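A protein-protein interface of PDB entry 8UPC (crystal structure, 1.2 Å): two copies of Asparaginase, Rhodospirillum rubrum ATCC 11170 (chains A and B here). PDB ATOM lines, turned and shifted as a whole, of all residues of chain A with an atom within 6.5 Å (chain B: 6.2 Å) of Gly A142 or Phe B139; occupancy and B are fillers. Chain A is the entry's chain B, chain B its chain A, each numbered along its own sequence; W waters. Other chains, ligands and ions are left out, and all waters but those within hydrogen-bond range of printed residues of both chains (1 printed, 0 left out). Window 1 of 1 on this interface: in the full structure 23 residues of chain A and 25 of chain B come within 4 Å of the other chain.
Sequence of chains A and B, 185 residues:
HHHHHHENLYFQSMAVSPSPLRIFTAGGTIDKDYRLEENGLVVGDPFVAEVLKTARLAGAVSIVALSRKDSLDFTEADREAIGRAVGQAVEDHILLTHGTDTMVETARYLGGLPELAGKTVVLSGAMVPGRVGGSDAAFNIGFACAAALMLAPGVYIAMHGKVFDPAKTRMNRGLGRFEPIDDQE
The backbone NH of Ala B137 sits at hydrogen-bond distance from the side-chain hydroxyl of Ser B135 (2.9 Å).
The side-chain carboxylate (OD2) of Asp B136 sits at hydrogen-bond distance from the side-chain amide nitrogen (ND2) of Asn B140 (3.1 Å).
The side-chain hydroxyl (OG1) of Thr A54 is in hydrogen-bond range of the backbone carbonyl oxygen (O) of Val A51 (3.3 Å).
Among the printed residues, merely in contact across the chains: Val A51 with Phe B139, Leu A52 with Phe B139, Thr A54 with Ser B135, Thr A54 with Asp B136, Ala A55 with Phe B139, Ala A55 with His B160, Leu A57 with His B160, Ala A138 with Ala B138, Phe A139 with Val B51, Phe A139 with Ala B138, Phe A139 with Gly B142, Gly A142 with Phe B139, Gly A142 with Gly B142, Gly A142 with Phe B143, Phe A143 with Gly B142, Phe A143 with Phe B143, Phe A143 with Ala B146, Ala A146 with Phe B143 and Ala A146 with Ala B146.
Printed residues of chain B within 4 Å of Ala A138: Ala B138.
Of the printed residues of chain B, Phe A139 touches Val B51, Ala B138 and Gly B142.
Printed residues of chain B within 4 Å of Gly A142: Phe B139 (3.5 Å), Gly B142 (3.5 Å) and Phe B143 (3.2 Å).
Of the printed residues of chain A, Val B51 touches Phe A139.
Printed residues of chain A within 4 Å of Phe B139: Val A51, Leu A52, Ala A55 and Gly A142.
Of the printed residues of chain A, Gly B142 touches Phe A139 (3.6 Å), Gly A142 (3.5 Å) and Phe A143 (3.2 Å).
Hydrophobic or aromatic side chains of chain A that line the printed part of chain B: Val A51, Leu A52, Ala A55, Leu A57, Ala A138, Phe A139, Phe A143 and Ala A146.
Among the printed residues, 19 pairs touch across the chains.
Among the printed residues, no Asp or Glu carboxylate lies within 4 Å of a Lys or Arg side-chain nitrogen of the other chain.
Val A51 touches Phe B139, and with the chains exchanged Phe A139 touches Val B51.
Phe A139 touches Ala B138, but with the chains exchanged Ala A138 does not touch Phe B139 (4.001 Å).
Phe A143 touches Ala B146, and with the chains exchanged Ala A146 touches Phe B143.
Ala A146 touches its own counterpart, Ala B146.
Positions printed for both chains: 51, 137, 138, 139, 140, 141, 142, 143, 144 and 146.
Of the 19 pairs that touch across the chains among the printed residues, 12 have their exchanged pair printed and touching as well.
Water W1 lies within hydrogen-bond range of O of Thr A54 and N of Asp B136.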
ATOM      1  N   VAL A  51      26.094  21.652 -14.881  1.00  0.00           N
ATOM      2  CA  VAL A  51      26.648  22.864 -14.241  1.00  0.00           C
ATOM      3  C   VAL A  51      28.158  22.817 -14.298  1.00  0.00           C
ATOM      4  O   VAL A  51      28.808  23.833 -14.603  1.00  0.00           O
ATOM      5  CB  VAL A  51      26.142  22.978 -12.797  1.00  0.00           C
ATOM      6  CG1 VAL A  51      26.780  24.172 -12.098  1.00  0.00           C
ATOM      7  CG2 VAL A  51      24.632  23.105 -12.837  1.00  0.00           C
ATOM      8  N   LEU A  52      28.771  21.674 -14.002  1.00  0.00           N
ATOM      9  CA  LEU A  52      30.236  21.648 -13.947  1.00  0.00           C
ATOM     10  C   LEU A  52      30.848  21.698 -15.354  1.00  0.00           C
ATOM     11  O   LEU A  52      31.961  22.225 -15.463  1.00  0.00           O
ATOM     12  CB  LEU A  52      30.732  20.440 -13.152  1.00  0.00           C
ATOM     13  CG  LEU A  52      30.364  20.465 -11.681  1.00  0.00           C
ATOM     14  CD1 LEU A  52      30.974  19.293 -10.954  1.00  0.00           C
ATOM     15  CD2 LEU A  52      30.673  21.777 -10.974  1.00  0.00           C
ATOM     16  N   THR A  54      30.306  23.824 -17.646  1.00  0.00           N
ATOM     17  CA  THR A  54      30.523  25.244 -17.978  1.00  0.00           C
ATOM     18  C   THR A  54      31.220  25.982 -16.836  1.00  0.00           C
ATOM     19  O   THR A  54      31.430  27.191 -16.939  1.00  0.00           O
ATOM     20  CB  THR A  54      29.195  25.903 -18.363  1.00  0.00           C
ATOM     21  OG1 THR A  54      28.281  25.732 -17.281  1.00  0.00           O
ATOM     22  CG2 THR A  54      28.622  25.322 -19.630  1.00  0.00           C
ATOM     23  N   ALA A  55      31.643  25.304 -15.773  1.00  0.00           N
ATOM     24  CA  ALA A  55      32.227  25.968 -14.595  1.00  0.00           C
ATOM     25  C   ALA A  55      33.690  26.314 -14.795  1.00  0.00           C
ATOM     26  O   ALA A  55      34.235  26.994 -13.920  1.00  0.00           O
ATOM     27  CB  ALA A  55      32.019  25.124 -13.373  1.00  0.00           C
ATOM     28  N   LEU A  57      36.459  24.598 -14.462  1.00  0.00           N
ATOM     29  CA  LEU A  57      37.139  24.191 -13.220  1.00  0.00           C
ATOM     30  C   LEU A  57      38.649  24.155 -13.373  1.00  0.00           C
ATOM     31  O   LEU A  57      39.159  23.656 -14.392  1.00  0.00           O
ATOM     32  CB  LEU A  57      36.639  22.830 -12.798  1.00  0.00           C
ATOM     33  CG  LEU A  57      35.159  22.765 -12.432  1.00  0.00           C
ATOM     34  CD1 LEU A  57      34.829  21.331 -12.099  1.00  0.00           C
ATOM     35  CD2 LEU A  57      34.826  23.693 -11.288  1.00  0.00           C
ATOM     36  N   ALA A 137      19.238  25.312  -8.588  1.00  0.00           N
ATOM     37  CA  ALA A 137      20.229  24.212  -8.687  1.00  0.00           C
ATOM     38  C   ALA A 137      21.663  24.692  -8.881  1.00  0.00           C
ATOM     39  O   ALA A 137      22.572  24.202  -8.186  1.00  0.00           O
ATOM     40  CB  ALA A 137      19.846  23.261  -9.775  1.00  0.00           C
ATOM     41  N   ALA A 138      21.944  25.571  -9.849  1.00  0.00           N
ATOM     42  CA  ALA A 138      23.345  25.942 -10.146  1.00  0.00           C
ATOM     43  C   ALA A 138      23.982  26.666  -8.966  1.00  0.00           C
ATOM     44  O   ALA A 138      25.122  26.354  -8.577  1.00  0.00           O
ATOM     45  CB  ALA A 138      23.424  26.786 -11.401  1.00  0.00           C
ATOM     46  N   PHE A 139      23.255  27.574  -8.320  1.00  0.00           N
ATOM     47  CA  PHE A 139      23.739  28.238  -7.107  1.00  0.00           C
ATOM     48  C   PHE A 139      24.023  27.177  -6.047  1.00  0.00           C
ATOM     49  O   PHE A 139      25.095  27.194  -5.398  1.00  0.00           O
ATOM     50  CB  PHE A 139      22.692  29.229  -6.593  1.00  0.00           C
ATOM     51  CG  PHE A 139      23.039  29.843  -5.264  1.00  0.00           C
ATOM     52  CD1 PHE A 139      23.839  30.962  -5.215  1.00  0.00           C
ATOM     53  CD2 PHE A 139      22.630  29.242  -4.090  1.00  0.00           C
ATOM     54  CE1 PHE A 139      24.183  31.504  -3.980  1.00  0.00           C
ATOM     55  CE2 PHE A 139      23.013  29.776  -2.870  1.00  0.00           C
ATOM     56  CZ  PHE A 139      23.771  30.910  -2.827  1.00  0.00           C
ATOM     57  N   ASN A 140      23.087  26.248  -5.846  1.00  0.00           N
ATOM     58  CA  ASN A 140      23.262  25.242  -4.789  1.00  0.00           C
ATOM     59  C   ASN A 140      24.473  24.380  -5.052  1.00  0.00           C
ATOM     60  O   ASN A 140      25.204  24.005  -4.111  1.00  0.00           O
ATOM     61  CB  ASN A 140      22.047  24.346  -4.650  1.00  0.00           C
ATOM     62  CG  ASN A 140      20.830  25.030  -4.091  1.00  0.00           C
ATOM     63  OD1 ASN A 140      20.961  26.135  -3.534  1.00  0.00           O
ATOM     64  ND2 ASN A 140      19.679  24.397  -4.239  1.00  0.00           N
ATOM     65  N   ILE A 141      24.722  24.021  -6.312  1.00  0.00           N
ATOM     66  CA  ILE A 141      25.917  23.220  -6.649  1.00  0.00           C
ATOM     67  C   ILE A 141      27.195  23.988  -6.349  1.00  0.00           C
ATOM     68  O   ILE A 141      28.119  23.424  -5.726  1.00  0.00           O
ATOM     69  CB  ILE A 141      25.837  22.758  -8.112  1.00  0.00           C
ATOM     70  CG1 ILE A 141      24.727  21.726  -8.272  1.00  0.00           C
ATOM     71  CG2 ILE A 141      27.171  22.223  -8.578  1.00  0.00           C
ATOM     72  CD1 ILE A 141      24.220  21.589  -9.675  1.00  0.00           C
ATOM     73  N   GLY A 142      27.293  25.254  -6.744  1.00  0.00           N
ATOM     74  CA  GLY A 142      28.510  26.018  -6.434  1.00  0.00           C
ATOM     75  C   GLY A 142      28.718  26.152  -4.926  1.00  0.00           C
ATOM     76  O   GLY A 142      29.826  25.911  -4.428  1.00  0.00           O
ATOM     77  N   PHE A 143      27.652  26.459  -4.190  1.00  0.00           N
ATOM     78  CA  PHE A 143      27.737  26.633  -2.728  1.00  0.00           C
ATOM     79  C   PHE A 143      28.151  25.313  -2.073  1.00  0.00           C
ATOM     80  O   PHE A 143      29.004  25.303  -1.178  1.00  0.00           O
ATOM     81  CB  PHE A 143      26.366  27.141  -2.249  1.00  0.00           C
ATOM     82  CG  PHE A 143      26.359  27.591  -0.811  1.00  0.00           C
ATOM     83  CD1 PHE A 143      26.239  26.665   0.215  1.00  0.00           C
ATOM     84  CD2 PHE A 143      26.451  28.921  -0.474  1.00  0.00           C
ATOM     85  CE1 PHE A 143      26.276  27.087   1.541  1.00  0.00           C
ATOM     86  CE2 PHE A 143      26.478  29.330   0.842  1.00  0.00           C
ATOM     87  CZ  PHE A 143      26.390  28.411   1.838  1.00  0.00           C
ATOM     88  N   ALA A 144      27.566  24.212  -2.526  1.00  0.00           N
ATOM     89  CA  ALA A 144      27.847  22.898  -1.916  1.00  0.00           C
ATOM     90  C   ALA A 144      29.239  22.391  -2.267  1.00  0.00           C
ATOM     91  O   ALA A 144      29.862  21.706  -1.418  1.00  0.00           O
ATOM     92  CB  ALA A 144      26.787  21.926  -2.297  1.00  0.00           C
ATOM     93  N   CYS A 145      29.754  22.668  -3.451  1.00  0.00           N
ATOM     94  CA  CYS A 145      31.142  22.328  -3.791  1.00  0.00           C
ATOM     95  C   CYS A 145      32.097  23.052  -2.865  1.00  0.00           C
ATOM     96  O   CYS A 145      33.030  22.413  -2.319  1.00  0.00           O
ATOM     97  CB  CYS A 145      31.457  22.640  -5.248  1.00  0.00           C
ATOM     98  SG  CYS A 145      30.749  21.503  -6.464  1.00  0.00           S
ATOM     99  N   ALA A 146      31.923  24.342  -2.672  1.00  0.00           N
ATOM    100  CA  ALA A 146      32.773  25.076  -1.731  1.00  0.00           C
ATOM    101  C   ALA A 146      32.624  24.494  -0.336  1.00  0.00           C
ATOM    102  O   ALA A 146      33.654  24.293   0.365  1.00  0.00           O
ATOM    103  CB  ALA A 146      32.437  26.552  -1.730  1.00  0.00           C
ATOM    104  N   ALA A 147      31.417  24.224   0.134  1.00  0.00           N
ATOM    105  CA  ALA A 147      31.199  23.664   1.474  1.00  0.00           C
ATOM    106  C   ALA A 147      31.941  22.344   1.615  1.00  0.00           C
ATOM    107  O   ALA A 147      32.586  22.098   2.663  1.00  0.00           O
ATOM    108  CB  ALA A 147      29.733  23.450   1.750  1.00  0.00           C
ATOM    109  N   VAL B  51      20.830  35.738  -9.710  1.00  0.00           N
ATOM    110  CA  VAL B  51      21.115  34.402  -9.160  1.00  0.00           C
ATOM    111  C   VAL B  51      20.531  34.285  -7.769  1.00  0.00           C
ATOM    112  O   VAL B  51      19.937  33.267  -7.424  1.00  0.00           O
ATOM    113  CB  VAL B  51      22.621  34.127  -9.177  1.00  0.00           C
ATOM    114  CG1 VAL B  51      22.929  32.787  -8.530  1.00  0.00           C
ATOM    115  CG2 VAL B  51      23.148  34.148 -10.607  1.00  0.00           C
ATOM    116  N   SER B 135      27.246  30.139 -19.292  1.00  0.00           N
ATOM    117  CA  SER B 135      28.077  30.929 -18.353  1.00  0.00           C
ATOM    118  C   SER B 135      28.410  30.157 -17.094  1.00  0.00           C
ATOM    119  O   SER B 135      27.574  29.418 -16.531  1.00  0.00           O
ATOM    120  CB  SER B 135      27.341  32.193 -17.996  1.00  0.00           C
ATOM    121  OG  SER B 135      28.044  32.941 -17.021  1.00  0.00           O
ATOM    122  N   ASP B 136      29.590  30.437 -16.579  1.00  0.00           N
ATOM    123  CA  ASP B 136      30.086  29.987 -15.259  1.00  0.00           C
ATOM    124  C   ASP B 136      29.527  30.815 -14.108  1.00  0.00           C
ATOM    125  O   ASP B 136      29.828  30.518 -12.962  1.00  0.00           O
ATOM    126  CB  ASP B 136      31.630  30.066 -15.280  1.00  0.00           C
ATOM    127  CG  ASP B 136      32.269  31.351 -15.785  1.00  0.00           C
ATOM    128  OD1 ASP B 136      31.692  32.029 -16.680  1.00  0.00           O
ATOM    129  OD2 ASP B 136      33.380  31.706 -15.297  1.00  0.00           O
ATOM    130  N   ALA B 137      28.781  31.881 -14.384  1.00  0.00           N
ATOM    131  CA  ALA B 137      28.450  32.875 -13.345  1.00  0.00           C
ATOM    132  C   ALA B 137      27.693  32.286 -12.172  1.00  0.00           C
ATOM    133  O   ALA B 137      28.046  32.571 -11.033  1.00  0.00           O
ATOM    134  CB  ALA B 137      27.680  34.006 -13.979  1.00  0.00           C
ATOM    135  N   ALA B 138      26.607  31.540 -12.388  1.00  0.00           N
ATOM    136  CA  ALA B 138      25.779  31.078 -11.248  1.00  0.00           C
ATOM    137  C   ALA B 138      26.575  30.152 -10.340  1.00  0.00           C
ATOM    138  O   ALA B 138      26.528  30.279  -9.102  1.00  0.00           O
ATOM    139  CB  ALA B 138      24.494  30.452 -11.723  1.00  0.00           C
ATOM    140  N   PHE B 139      27.330  29.216 -10.917  1.00  0.00           N
ATOM    141  CA  PHE B 139      28.217  28.357 -10.132  1.00  0.00           C
ATOM    142  C   PHE B 139      29.184  29.222  -9.324  1.00  0.00           C
ATOM    143  O   PHE B 139      29.398  28.984  -8.120  1.00  0.00           O
ATOM    144  CB  PHE B 139      28.964  27.400 -11.059  1.00  0.00           C
ATOM    145  CG  PHE B 139      29.993  26.571 -10.323  1.00  0.00           C
ATOM    146  CD1 PHE B 139      29.646  25.383  -9.724  1.00  0.00           C
ATOM    147  CD2 PHE B 139      31.302  27.018 -10.203  1.00  0.00           C
ATOM    148  CE1 PHE B 139      30.600  24.641  -9.030  1.00  0.00           C
ATOM    149  CE2 PHE B 139      32.251  26.301  -9.486  1.00  0.00           C
ATOM    150  CZ  PHE B 139      31.881  25.114  -8.898  1.00  0.00           C
ATOM    151  N   ASN B 140      29.836  30.177  -9.980  1.00  0.00           N
ATOM    152  CA  ASN B 140      30.857  31.001  -9.289  1.00  0.00           C
ATOM    153  C   ASN B 140      30.223  31.774  -8.155  1.00  0.00           C
ATOM    154  O   ASN B 140      30.854  31.936  -7.096  1.00  0.00           O
ATOM    155  CB  ASN B 140      31.560  31.956 -10.241  1.00  0.00           C
ATOM    156  CG  ASN B 140      32.458  31.300 -11.259  1.00  0.00           C
ATOM    157  OD1 ASN B 140      32.816  30.145 -11.090  1.00  0.00           O
ATOM    158  ND2 ASN B 140      32.809  32.060 -12.298  1.00  0.00           N
ATOM    159  N   ILE B 141      28.996  32.256  -8.344  1.00  0.00           N
ATOM    160  CA  ILE B 141      28.325  33.001  -7.269  1.00  0.00           C
ATOM    161  C   ILE B 141      28.037  32.075  -6.087  1.00  0.00           C
ATOM    162  O   ILE B 141      28.288  32.467  -4.938  1.00  0.00           O
ATOM    163  CB  ILE B 141      27.068  33.681  -7.818  1.00  0.00           C
ATOM    164  CG1 ILE B 141      27.409  34.821  -8.780  1.00  0.00           C
ATOM    165  CG2 ILE B 141      26.179  34.143  -6.666  1.00  0.00           C
ATOM    166  CD1 ILE B 141      28.318  35.881  -8.228  1.00  0.00           C
ATOM    167  N   GLY B 142      27.529  30.883  -6.327  1.00  0.00           N
ATOM    168  CA  GLY B 142      27.264  29.997  -5.189  1.00  0.00           C
ATOM    169  C   GLY B 142      28.549  29.651  -4.465  1.00  0.00           C
ATOM    170  O   GLY B 142      28.614  29.701  -3.229  1.00  0.00           O
ATOM    171  N   PHE B 143      29.591  29.311  -5.226  1.00  0.00           N
ATOM    172  CA  PHE B 143      30.892  28.949  -4.642  1.00  0.00           C
ATOM    173  C   PHE B 143      31.469  30.106  -3.832  1.00  0.00           C
ATOM    174  O   PHE B 143      31.974  29.902  -2.712  1.00  0.00           O
ATOM    175  CB  PHE B 143      31.821  28.502  -5.784  1.00  0.00           C
ATOM    176  CG  PHE B 143      33.108  27.876  -5.293  1.00  0.00           C
ATOM    177  CD1 PHE B 143      34.178  28.682  -4.928  1.00  0.00           C
ATOM    178  CD2 PHE B 143      33.250  26.497  -5.235  1.00  0.00           C
ATOM    179  CE1 PHE B 143      35.365  28.099  -4.494  1.00  0.00           C
ATOM    180  CE2 PHE B 143      34.444  25.931  -4.789  1.00  0.00           C
ATOM    181  CZ  PHE B 143      35.475  26.743  -4.403  1.00  0.00           C
ATOM    182  N   ALA B 144      31.392  31.307  -4.388  1.00  0.00           N
ATOM    183  CA  ALA B 144      31.992  32.475  -3.732  1.00  0.00           C
ATOM    184  C   ALA B 144      31.208  32.908  -2.499  1.00  0.00           C
ATOM    185  O   ALA B 144      31.801  33.434  -1.561  1.00  0.00           O
ATOM    186  CB  ALA B 144      32.104  33.605  -4.716  1.00  0.00           C
ATOM    187  N   ALA B 146      29.596  30.840  -0.478  1.00  0.00           N
ATOM    188  CA  ALA B 146      30.073  29.904   0.543  1.00  0.00           C
ATOM    189  C   ALA B 146      31.483  30.267   1.011  1.00  0.00           C
ATOM    190  O   ALA B 146      31.751  30.256   2.231  1.00  0.00           O
ATOM    191  CB  ALA B 146      30.056  28.509  -0.007  1.00  0.00           C
ATOM    192  N   HIS B 160      36.671  29.292 -10.791  1.00  0.00           N
ATOM    193  CA  HIS B 160      37.077  27.959 -11.294  1.00  0.00           C
ATOM    194  C   HIS B 160      36.973  26.903 -10.199  1.00  0.00           C
ATOM    195  O   HIS B 160      37.675  25.872 -10.290  1.00  0.00           O
ATOM    196  CB  HIS B 160      38.486  28.018 -11.894  1.00  0.00           C
ATOM    197  CG  HIS B 160      38.839  29.272 -12.629  1.00  0.00           C
ATOM    198  ND1 HIS B 160      38.044  29.845 -13.612  1.00  0.00           N
ATOM    199  CD2 HIS B 160      39.913  30.075 -12.499  1.00  0.00           C
ATOM    200  CE1 HIS B 160      38.671  30.947 -14.061  1.00  0.00           C
ATOM    201  NE2 HIS B 160      39.817  31.097 -13.396  1.00  0.00           N
ATOM    202  N   GLY B 161      36.081  27.090  -9.234  1.00  0.00           N
ATOM    203  CA  GLY B 161      35.930  26.107  -8.154  1.00  0.00           C
ATOM    204  C   GLY B 161      37.134  26.002  -7.242  1.00  0.00           C
ATOM    205  O   GLY B 161      37.323  24.973  -6.625  1.00  0.00           O
ATOM    206  N   LYS B 162      37.883  27.096  -7.151  1.00  0.00           N
ATOM    207  CA  LYS B 162      39.155  27.133  -6.427  1.00  0.00           C
ATOM    208  C   LYS B 162      39.305  28.461  -5.702  1.00  0.00           C
ATOM    209  O   LYS B 162      38.836  29.501  -6.194  1.00  0.00           O
ATOM    210  CB  LYS B 162      40.320  26.908  -7.442  1.00  0.00           C
ATOM    211  CG  LYS B 162      41.716  26.956  -6.906  1.00  0.00           C
ATOM    212  CD  LYS B 162      42.715  26.550  -7.951  1.00  0.00           C
ATOM    213  CE  LYS B 162      44.176  26.587  -7.495  1.00  0.00           C
ATOM    214  NZ  LYS B 162      44.422  25.671  -6.363  1.00  0.00           N
HETATM  215  O   HOH W   1      31.557  28.996 -18.990  1.00  0.00           O
